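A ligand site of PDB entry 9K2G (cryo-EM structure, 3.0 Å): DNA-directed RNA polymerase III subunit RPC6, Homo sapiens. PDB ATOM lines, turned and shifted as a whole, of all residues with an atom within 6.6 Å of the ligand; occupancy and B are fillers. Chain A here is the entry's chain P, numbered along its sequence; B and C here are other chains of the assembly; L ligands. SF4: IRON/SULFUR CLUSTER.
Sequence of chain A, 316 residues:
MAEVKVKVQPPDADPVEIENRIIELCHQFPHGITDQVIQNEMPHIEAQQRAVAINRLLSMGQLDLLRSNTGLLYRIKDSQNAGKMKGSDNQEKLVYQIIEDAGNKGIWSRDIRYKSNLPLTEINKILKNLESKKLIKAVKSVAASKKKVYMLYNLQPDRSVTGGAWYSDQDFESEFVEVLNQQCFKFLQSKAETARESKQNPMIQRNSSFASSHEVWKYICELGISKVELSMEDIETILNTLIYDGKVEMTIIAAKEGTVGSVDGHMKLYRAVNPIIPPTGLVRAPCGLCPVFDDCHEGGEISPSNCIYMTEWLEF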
ATOM      1  N   ALA A 285      24.080 -26.904  10.640  1.00  0.00           N
ATOM      2  CA  ALA A 285      22.919 -26.475  11.398  1.00  0.00           C
ATOM      3  C   ALA A 285      22.819 -24.957  11.399  1.00  0.00           C
ATOM      4  O   ALA A 285      23.849 -24.273  11.431  1.00  0.00           O
ATOM      5  CB  ALA A 285      22.992 -26.974  12.843  1.00  0.00           C
ATOM      6  N   PRO A 286      21.597 -24.400  11.339  1.00  0.00           N
ATOM      7  CA  PRO A 286      21.473 -22.935  11.324  1.00  0.00           C
ATOM      8  C   PRO A 286      22.048 -22.249  12.545  1.00  0.00           C
ATOM      9  O   PRO A 286      22.551 -21.130  12.429  1.00  0.00           O
ATOM     10  CB  PRO A 286      19.946 -22.731  11.229  1.00  0.00           C
ATOM     11  CG  PRO A 286      19.416 -24.012  10.679  1.00  0.00           C
ATOM     12  CD  PRO A 286      20.299 -25.084  11.240  1.00  0.00           C
ATOM     13  N   CYS A 287      21.996 -22.897  13.710  1.00  0.00           N
ATOM     14  CA  CYS A 287      22.532 -22.276  14.927  1.00  0.00           C
ATOM     15  C   CYS A 287      24.040 -22.074  14.825  1.00  0.00           C
ATOM     16  O   CYS A 287      24.582 -21.156  15.469  1.00  0.00           O
ATOM     17  CB  CYS A 287      22.189 -23.138  16.138  1.00  0.00           C
ATOM     18  SG  CYS A 287      20.426 -23.436  16.358  1.00  0.00           S
ATOM     19  N   GLY A 288      24.727 -22.890  14.031  1.00  0.00           N
ATOM     20  CA  GLY A 288      26.154 -22.702  13.821  1.00  0.00           C
ATOM     21  C   GLY A 288      26.493 -21.486  12.983  1.00  0.00           C
ATOM     22  O   GLY A 288      27.619 -20.991  13.056  1.00  0.00           O
ATOM     23  N   LEU A 289      25.545 -21.006  12.176  1.00  0.00           N
ATOM     24  CA  LEU A 289      25.743 -19.834  11.343  1.00  0.00           C
ATOM     25  C   LEU A 289      24.855 -18.659  11.747  1.00  0.00           C
ATOM     26  O   LEU A 289      24.847 -17.639  11.045  1.00  0.00           O
ATOM     27  CB  LEU A 289      25.497 -20.176   9.868  1.00  0.00           C
ATOM     28  CG  LEU A 289      26.257 -21.381   9.311  1.00  0.00           C
ATOM     29  CD1 LEU A 289      25.998 -21.535   7.821  1.00  0.00           C
ATOM     30  CD2 LEU A 289      27.753 -21.270   9.598  1.00  0.00           C
ATOM     31  N   CYS A 290      24.122 -18.782  12.840  1.00  0.00           N
ATOM     32  CA  CYS A 290      23.201 -17.716  13.241  1.00  0.00           C
ATOM     33  C   CYS A 290      23.982 -16.472  13.673  1.00  0.00           C
ATOM     34  O   CYS A 290      24.893 -16.573  14.489  1.00  0.00           O
ATOM     35  CB  CYS A 290      22.313 -18.187  14.381  1.00  0.00           C
ATOM     36  SG  CYS A 290      21.362 -16.854  15.147  1.00  0.00           S
ATOM     37  N   PRO A 291      23.633 -15.296  13.143  1.00  0.00           N
ATOM     38  CA  PRO A 291      24.335 -14.073  13.573  1.00  0.00           C
ATOM     39  C   PRO A 291      23.859 -13.529  14.902  1.00  0.00           C
ATOM     40  O   PRO A 291      24.567 -12.701  15.489  1.00  0.00           O
ATOM     41  CB  PRO A 291      24.028 -13.089  12.430  1.00  0.00           C
ATOM     42  CG  PRO A 291      22.672 -13.512  11.964  1.00  0.00           C
ATOM     43  CD  PRO A 291      22.624 -15.018  12.113  1.00  0.00           C
ATOM     44  N   VAL A 292      22.692 -13.951  15.391  1.00  0.00           N
ATOM     45  CA  VAL A 292      22.139 -13.443  16.637  1.00  0.00           C
ATOM     46  C   VAL A 292      22.156 -14.580  17.657  1.00  0.00           C
ATOM     47  O   VAL A 292      21.326 -14.638  18.572  1.00  0.00           O
ATOM     48  CB  VAL A 292      20.736 -12.852  16.407  1.00  0.00           C
ATOM     49  CG1 VAL A 292      19.680 -13.941  16.142  1.00  0.00           C
ATOM     50  CG2 VAL A 292      20.337 -11.924  17.559  1.00  0.00           C
ATOM     51  N   PHE A 293      23.126 -15.481  17.509  1.00  0.00           N
ATOM     52  CA  PHE A 293      23.249 -16.645  18.381  1.00  0.00           C
ATOM     53  C   PHE A 293      23.325 -16.243  19.856  1.00  0.00           C
ATOM     54  O   PHE A 293      22.824 -16.962  20.736  1.00  0.00           O
ATOM     55  CB  PHE A 293      24.481 -17.465  17.980  1.00  0.00           C
ATOM     56  CG  PHE A 293      24.872 -18.515  18.987  1.00  0.00           C
ATOM     57  CD1 PHE A 293      24.220 -19.734  19.020  1.00  0.00           C
ATOM     58  CD2 PHE A 293      25.914 -18.292  19.874  1.00  0.00           C
ATOM     59  CE1 PHE A 293      24.593 -20.706  19.932  1.00  0.00           C
ATOM     60  CE2 PHE A 293      26.283 -19.256  20.782  1.00  0.00           C
ATOM     61  CZ  PHE A 293      25.620 -20.467  20.815  1.00  0.00           C
ATOM     62  N   ASP A 294      23.966 -15.107  20.154  1.00  0.00           N
ATOM     63  CA  ASP A 294      24.101 -14.666  21.537  1.00  0.00           C
ATOM     64  C   ASP A 294      22.742 -14.360  22.159  1.00  0.00           C
ATOM     65  O   ASP A 294      22.508 -14.677  23.330  1.00  0.00           O
ATOM     66  CB  ASP A 294      25.018 -13.442  21.610  1.00  0.00           C
ATOM     67  CG  ASP A 294      26.482 -13.812  21.510  1.00  0.00           C
ATOM     68  OD1 ASP A 294      26.952 -14.612  22.352  1.00  0.00           O
ATOM     69  OD2 ASP A 294      27.167 -13.319  20.591  1.00  0.00           O
ATOM     70  N   ASP A 295      21.845 -13.745  21.394  1.00  0.00           N
ATOM     71  CA  ASP A 295      20.546 -13.353  21.918  1.00  0.00           C
ATOM     72  C   ASP A 295      19.523 -14.474  21.930  1.00  0.00           C
ATOM     73  O   ASP A 295      18.413 -14.277  22.432  1.00  0.00           O
ATOM     74  CB  ASP A 295      19.996 -12.167  21.114  1.00  0.00           C
ATOM     75  CG  ASP A 295      20.810 -10.907  21.300  1.00  0.00           C
ATOM     76  OD1 ASP A 295      21.100 -10.554  22.464  1.00  0.00           O
ATOM     77  OD2 ASP A 295      21.145 -10.260  20.289  1.00  0.00           O
ATOM     78  N   CYS A 296      19.863 -15.638  21.375  1.00  0.00           N
ATOM     79  CA  CYS A 296      18.931 -16.755  21.367  1.00  0.00           C
ATOM     80  C   CYS A 296      18.686 -17.257  22.781  1.00  0.00           C
ATOM     81  O   CYS A 296      19.625 -17.458  23.560  1.00  0.00           O
ATOM     82  CB  CYS A 296      19.459 -17.886  20.495  1.00  0.00           C
ATOM     83  SG  CYS A 296      18.377 -19.334  20.443  1.00  0.00           S
ATOM     84  N   HIS A 297      17.416 -17.447  23.125  1.00  0.00           N
ATOM     85  CA  HIS A 297      17.016 -17.869  24.469  1.00  0.00           C
ATOM     86  C   HIS A 297      15.767 -18.718  24.353  1.00  0.00           C
ATOM     87  O   HIS A 297      15.005 -18.601  23.393  1.00  0.00           O
ATOM     88  CB  HIS A 297      16.787 -16.657  25.378  1.00  0.00           C
ATOM     89  CG  HIS A 297      16.410 -17.006  26.780  1.00  0.00           C
ATOM     90  ND1 HIS A 297      16.987 -18.064  27.460  1.00  0.00           N
ATOM     91  CD2 HIS A 297      15.531 -16.448  27.641  1.00  0.00           C
ATOM     92  CE1 HIS A 297      16.463 -18.126  28.673  1.00  0.00           C
ATOM     93  NE2 HIS A 297      15.583 -17.158  28.811  1.00  0.00           N
ATOM     94  N   ILE A 302      13.646 -14.045  20.540  1.00  0.00           N
ATOM     95  CA  ILE A 302      14.441 -14.878  19.643  1.00  0.00           C
ATOM     96  C   ILE A 302      14.570 -16.243  20.311  1.00  0.00           C
ATOM     97  O   ILE A 302      15.415 -16.435  21.192  1.00  0.00           O
ATOM     98  CB  ILE A 302      15.803 -14.248  19.349  1.00  0.00           C
ATOM     99  CG1 ILE A 302      15.610 -12.814  18.833  1.00  0.00           C
ATOM    100  CG2 ILE A 302      16.560 -15.076  18.324  1.00  0.00           C
ATOM    101  CD1 ILE A 302      16.915 -12.070  18.631  1.00  0.00           C
ATOM    102  N   SER A 303      13.747 -17.186  19.880  1.00  0.00           N
ATOM    103  CA  SER A 303      13.700 -18.520  20.467  1.00  0.00           C
ATOM    104  C   SER A 303      13.790 -19.570  19.372  1.00  0.00           C
ATOM    105  O   SER A 303      13.354 -19.343  18.239  1.00  0.00           O
ATOM    106  CB  SER A 303      12.388 -18.719  21.250  1.00  0.00           C
ATOM    107  OG  SER A 303      12.282 -20.022  21.780  1.00  0.00           O
ATOM    108  N   PRO A 304      14.381 -20.730  19.677  1.00  0.00           N
ATOM    109  CA  PRO A 304      14.439 -21.802  18.663  1.00  0.00           C
ATOM    110  C   PRO A 304      13.072 -22.271  18.207  1.00  0.00           C
ATOM    111  O   PRO A 304      12.942 -22.718  17.057  1.00  0.00           O
ATOM    112  CB  PRO A 304      15.208 -22.916  19.382  1.00  0.00           C
ATOM    113  CG  PRO A 304      15.115 -22.590  20.844  1.00  0.00           C
ATOM    114  CD  PRO A 304      15.090 -21.091  20.914  1.00  0.00           C
ATOM    115  N   SER A 305      12.050 -22.187  19.065  1.00  0.00           N
ATOM    116  CA  SER A 305      10.705 -22.611  18.659  1.00  0.00           C
ATOM    117  C   SER A 305      10.176 -21.751  17.521  1.00  0.00           C
ATOM    118  O   SER A 305       9.567 -22.262  16.573  1.00  0.00           O
ATOM    119  CB  SER A 305       9.764 -22.569  19.855  1.00  0.00           C
ATOM    120  OG  SER A 305       9.440 -21.229  20.196  1.00  0.00           O
ATOM    121  N   CYS A 307      12.178 -19.626  15.676  1.00  0.00           N
ATOM    122  CA  CYS A 307      13.322 -19.130  14.917  1.00  0.00           C
ATOM    123  C   CYS A 307      13.049 -19.209  13.421  1.00  0.00           C
ATOM    124  O   CYS A 307      12.586 -20.230  12.912  1.00  0.00           O
ATOM    125  CB  CYS A 307      14.580 -19.922  15.271  1.00  0.00           C
ATOM    126  SG  CYS A 307      16.050 -19.389  14.360  1.00  0.00           S
ATOM    127  N   ILE A 308      13.340 -18.117  12.713  1.00  0.00           N
ATOM    128  CA  ILE A 308      13.092 -18.051  11.277  1.00  0.00           C
ATOM    129  C   ILE A 308      14.100 -18.900  10.510  1.00  0.00           C
ATOM    130  O   ILE A 308      13.770 -19.502   9.480  1.00  0.00           O
ATOM    131  CB  ILE A 308      13.101 -16.586  10.800  1.00  0.00           C
ATOM    132  CG1 ILE A 308      11.973 -15.801  11.460  1.00  0.00           C
ATOM    133  CG2 ILE A 308      12.988 -16.492   9.282  1.00  0.00           C
ATOM    134  CD1 ILE A 308      10.597 -16.360  11.171  1.00  0.00           C
ATOM    135  N   TYR A 309      15.345 -18.956  10.986  1.00  0.00           N
ATOM    136  CA  TYR A 309      16.397 -19.640  10.256  1.00  0.00           C
ATOM    137  C   TYR A 309      16.070 -21.121  10.080  1.00  0.00           C
ATOM    138  O   TYR A 309      16.174 -21.663   8.975  1.00  0.00           O
ATOM    139  CB  TYR A 309      17.736 -19.453  10.963  1.00  0.00           C
ATOM    140  CG  TYR A 309      18.158 -18.013  11.071  1.00  0.00           C
ATOM    141  CD1 TYR A 309      18.740 -17.357   9.989  1.00  0.00           C
ATOM    142  CD2 TYR A 309      17.963 -17.298  12.245  1.00  0.00           C
ATOM    143  CE1 TYR A 309      19.114 -16.024  10.088  1.00  0.00           C
ATOM    144  CE2 TYR A 309      18.337 -15.966  12.343  1.00  0.00           C
ATOM    145  CZ  TYR A 309      18.910 -15.338  11.259  1.00  0.00           C
ATOM    146  OH  TYR A 309      19.283 -14.019  11.353  1.00  0.00           O
ATOM    147  N   MET A 310      15.663 -21.787  11.164  1.00  0.00           N
ATOM    148  CA  MET A 310      15.268 -23.182  11.052  1.00  0.00           C
ATOM    149  C   MET A 310      13.986 -23.344  10.250  1.00  0.00           C
ATOM    150  O   MET A 310      13.812 -24.361   9.577  1.00  0.00           O
ATOM    151  CB  MET A 310      15.125 -23.800  12.433  1.00  0.00           C
ATOM    152  CG  MET A 310      16.314 -24.647  12.855  1.00  0.00           C
ATOM    153  SD  MET A 310      16.561 -24.613  14.625  1.00  0.00           S
ATOM    154  CE  MET A 310      16.789 -22.853  14.880  1.00  0.00           C
ATOM    155  N   ARG B 438      29.524 -23.347  21.753  1.00  0.00           N
ATOM    156  CA  ARG B 438      28.528 -23.022  20.737  1.00  0.00           C
ATOM    157  C   ARG B 438      27.860 -24.269  20.178  1.00  0.00           C
ATOM    158  O   ARG B 438      26.656 -24.268  19.926  1.00  0.00           O
ATOM    159  CB  ARG B 438      29.181 -22.202  19.617  1.00  0.00           C
ATOM    160  CG  ARG B 438      28.278 -22.001  18.408  1.00  0.00           C
ATOM    161  CD  ARG B 438      28.977 -21.205  17.321  1.00  0.00           C
ATOM    162  NE  ARG B 438      29.075 -19.793  17.649  1.00  0.00           N
ATOM    163  CZ  ARG B 438      28.186 -18.877  17.286  1.00  0.00           C
ATOM    164  NH1 ARG B 438      27.117 -19.205  16.572  1.00  0.00           N
ATOM    165  NH2 ARG B 438      28.372 -17.610  17.631  1.00  0.00           N
ATOM    166  N   LYS B 441      25.272 -25.501  22.667  1.00  0.00           N
ATOM    167  CA  LYS B 441      24.031 -24.739  22.583  1.00  0.00           C
ATOM    168  C   LYS B 441      23.284 -25.013  21.283  1.00  0.00           C
ATOM    169  O   LYS B 441      22.048 -24.995  21.267  1.00  0.00           O
ATOM    170  CB  LYS B 441      24.312 -23.234  22.725  1.00  0.00           C
ATOM    171  CG  LYS B 441      23.050 -22.382  22.771  1.00  0.00           C
ATOM    172  CD  LYS B 441      23.314 -21.010  23.345  1.00  0.00           C
ATOM    173  CE  LYS B 441      22.048 -20.173  23.339  1.00  0.00           C
ATOM    174  NZ  LYS B 441      22.241 -18.811  23.927  1.00  0.00           N
ATOM    175  N   SER B 442      24.000 -25.278  20.186  1.00  0.00           N
ATOM    176  CA  SER B 442      23.349 -25.573  18.907  1.00  0.00           C
ATOM    177  C   SER B 442      22.556 -26.867  18.978  1.00  0.00           C
ATOM    178  O   SER B 442      21.413 -26.945  18.506  1.00  0.00           O
ATOM    179  CB  SER B 442      24.397 -25.639  17.793  1.00  0.00           C
ATOM    180  OG  SER B 442      23.888 -26.278  16.639  1.00  0.00           O
ATOM    181  N   ASN B 445      19.484 -26.301  20.998  1.00  0.00           N
ATOM    182  CA  ASN B 445      18.455 -25.616  20.222  1.00  0.00           C
ATOM    183  C   ASN B 445      17.767 -26.573  19.247  1.00  0.00           C
ATOM    184  O   ASN B 445      16.543 -26.501  19.060  1.00  0.00           O
ATOM    185  CB  ASN B 445      19.047 -24.429  19.478  1.00  0.00           C
ATOM    186  CG  ASN B 445      19.450 -23.293  20.403  1.00  0.00           C
ATOM    187  OD1 ASN B 445      19.013 -23.244  21.552  1.00  0.00           O
ATOM    188  ND2 ASN B 445      20.278 -22.389  19.905  1.00  0.00           N
ATOM    189  N   LEU B 446      18.529 -27.462  18.608  1.00  0.00           N
ATOM    190  CA  LEU B 446      17.923 -28.429  17.692  1.00  0.00           C
ATOM    191  C   LEU B 446      16.958 -29.342  18.439  1.00  0.00           C
ATOM    192  O   LEU B 446      15.838 -29.602  17.961  1.00  0.00           O
ATOM    193  CB  LEU B 446      19.009 -29.239  16.991  1.00  0.00           C
ATOM    194  CG  LEU B 446      19.883 -28.502  15.977  1.00  0.00           C
ATOM    195  CD1 LEU B 446      20.859 -29.459  15.310  1.00  0.00           C
ATOM    196  CD2 LEU B 446      19.025 -27.790  14.936  1.00  0.00           C
ATOM    197  N   PHE C  38      15.189 -11.135  13.169  1.00  0.00           N
ATOM    198  CA  PHE C  38      16.083 -12.126  12.575  1.00  0.00           C
ATOM    199  C   PHE C  38      16.699 -11.517  11.315  1.00  0.00           C
ATOM    200  O   PHE C  38      16.125 -11.622  10.223  1.00  0.00           O
ATOM    201  CB  PHE C  38      15.329 -13.420  12.241  1.00  0.00           C
ATOM    202  CG  PHE C  38      14.739 -14.103  13.447  1.00  0.00           C
ATOM    203  CD1 PHE C  38      13.485 -13.755  13.916  1.00  0.00           C
ATOM    204  CD2 PHE C  38      15.432 -15.102  14.100  1.00  0.00           C
ATOM    205  CE1 PHE C  38      12.931 -14.380  15.015  1.00  0.00           C
ATOM    206  CE2 PHE C  38      14.897 -15.738  15.210  1.00  0.00           C
ATOM    207  CZ  PHE C  38      13.645 -15.372  15.665  1.00  0.00           C
HETATM  208 FE1  SF4 L   1      20.250 -18.665  15.917  1.00  0.00          FE
HETATM  209 FE2  SF4 L   1      18.996 -19.265  18.267  1.00  0.00          FE
HETATM  210 FE3  SF4 L   1      19.787 -21.272  16.593  1.00  0.00          FE
HETATM  211 FE4  SF4 L   1      17.699 -19.646  15.877  1.00  0.00          FE
HETATM  212  S1  SF4 L   1      17.780 -21.093  17.653  1.00  0.00           S
HETATM  213  S2  SF4 L   1      19.445 -20.301  14.560  1.00  0.00           S
HETATM  214  S3  SF4 L   1      18.393 -17.657  16.755  1.00  0.00           S
HETATM  215  S4  SF4 L   1      21.130 -19.799  17.693  1.00  0.00           S
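An iron atom (FE3) of the ligand is bound by the side-chain sulfur of Cys 287. An iron atom (FE1) of the ligand is bound by the side-chain sulfur of Cys 290, at 2.3 Å. SG of Cys 296 is bound to FE2 of the ligand (2.3 Å). S2 of the ligand lies close to N of Cys 287. ND2 of Asn 445 of chain B lies close to S4 of the ligand, 3.5 Å away. An iron atom (FE4) of the ligand is bound by the side-chain sulfur (SG) of Cys 307 (2.3 Å).
The side-chain sulfur (SG) of Cys 290 lies close to the backbone NH (N) of Phe 293, 3.3 Å away. The side-chain amino group (NZ) of Lys 441 of chain B sits at hydrogen-bond distance from the backbone carbonyl oxygen (O) of Cys 296 (3.0 Å). SG of Cys 296 sits close to ND2 of Asn 445 of chain B. The backbone carbonyl oxygen of Ile 302 sits at hydrogen-bond distance from the backbone NH of His 297 (3.0 Å). The side-chain sulfur of Cys 287 lies close to the side-chain amide nitrogen of Asn 445 of chain B (3.7 Å). The side-chain sulfur (SG) of Cys 290 lies close to the backbone NH (N) of Val 292. The backbone carbonyl oxygen of Lys 441 of chain B sits close to the side-chain amide nitrogen of Asn 445 of chain B (3.4 Å). N of Tyr 309 lies close to SG of Cys 307 (3.5 Å).
Pro 286 touches the ligand (C to S2, 3.8 Å). Val 292 touches the ligand (CG1 to S3, 3.98 Å). Phe 293 touches the ligand. Ile 302 touches the ligand. CA of Pro 304 touches S1 of the ligand, at 3.6 Å. CE of Met 310 touches S1 of the ligand, at 3.4 Å. Hydrophobic or aromatic side chains that line the ligand: Val 292, Phe 293, Ile 302, Pro 304 and Met 310. Of the 27 residues printed, 11 come within 4 Å of the ligand.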
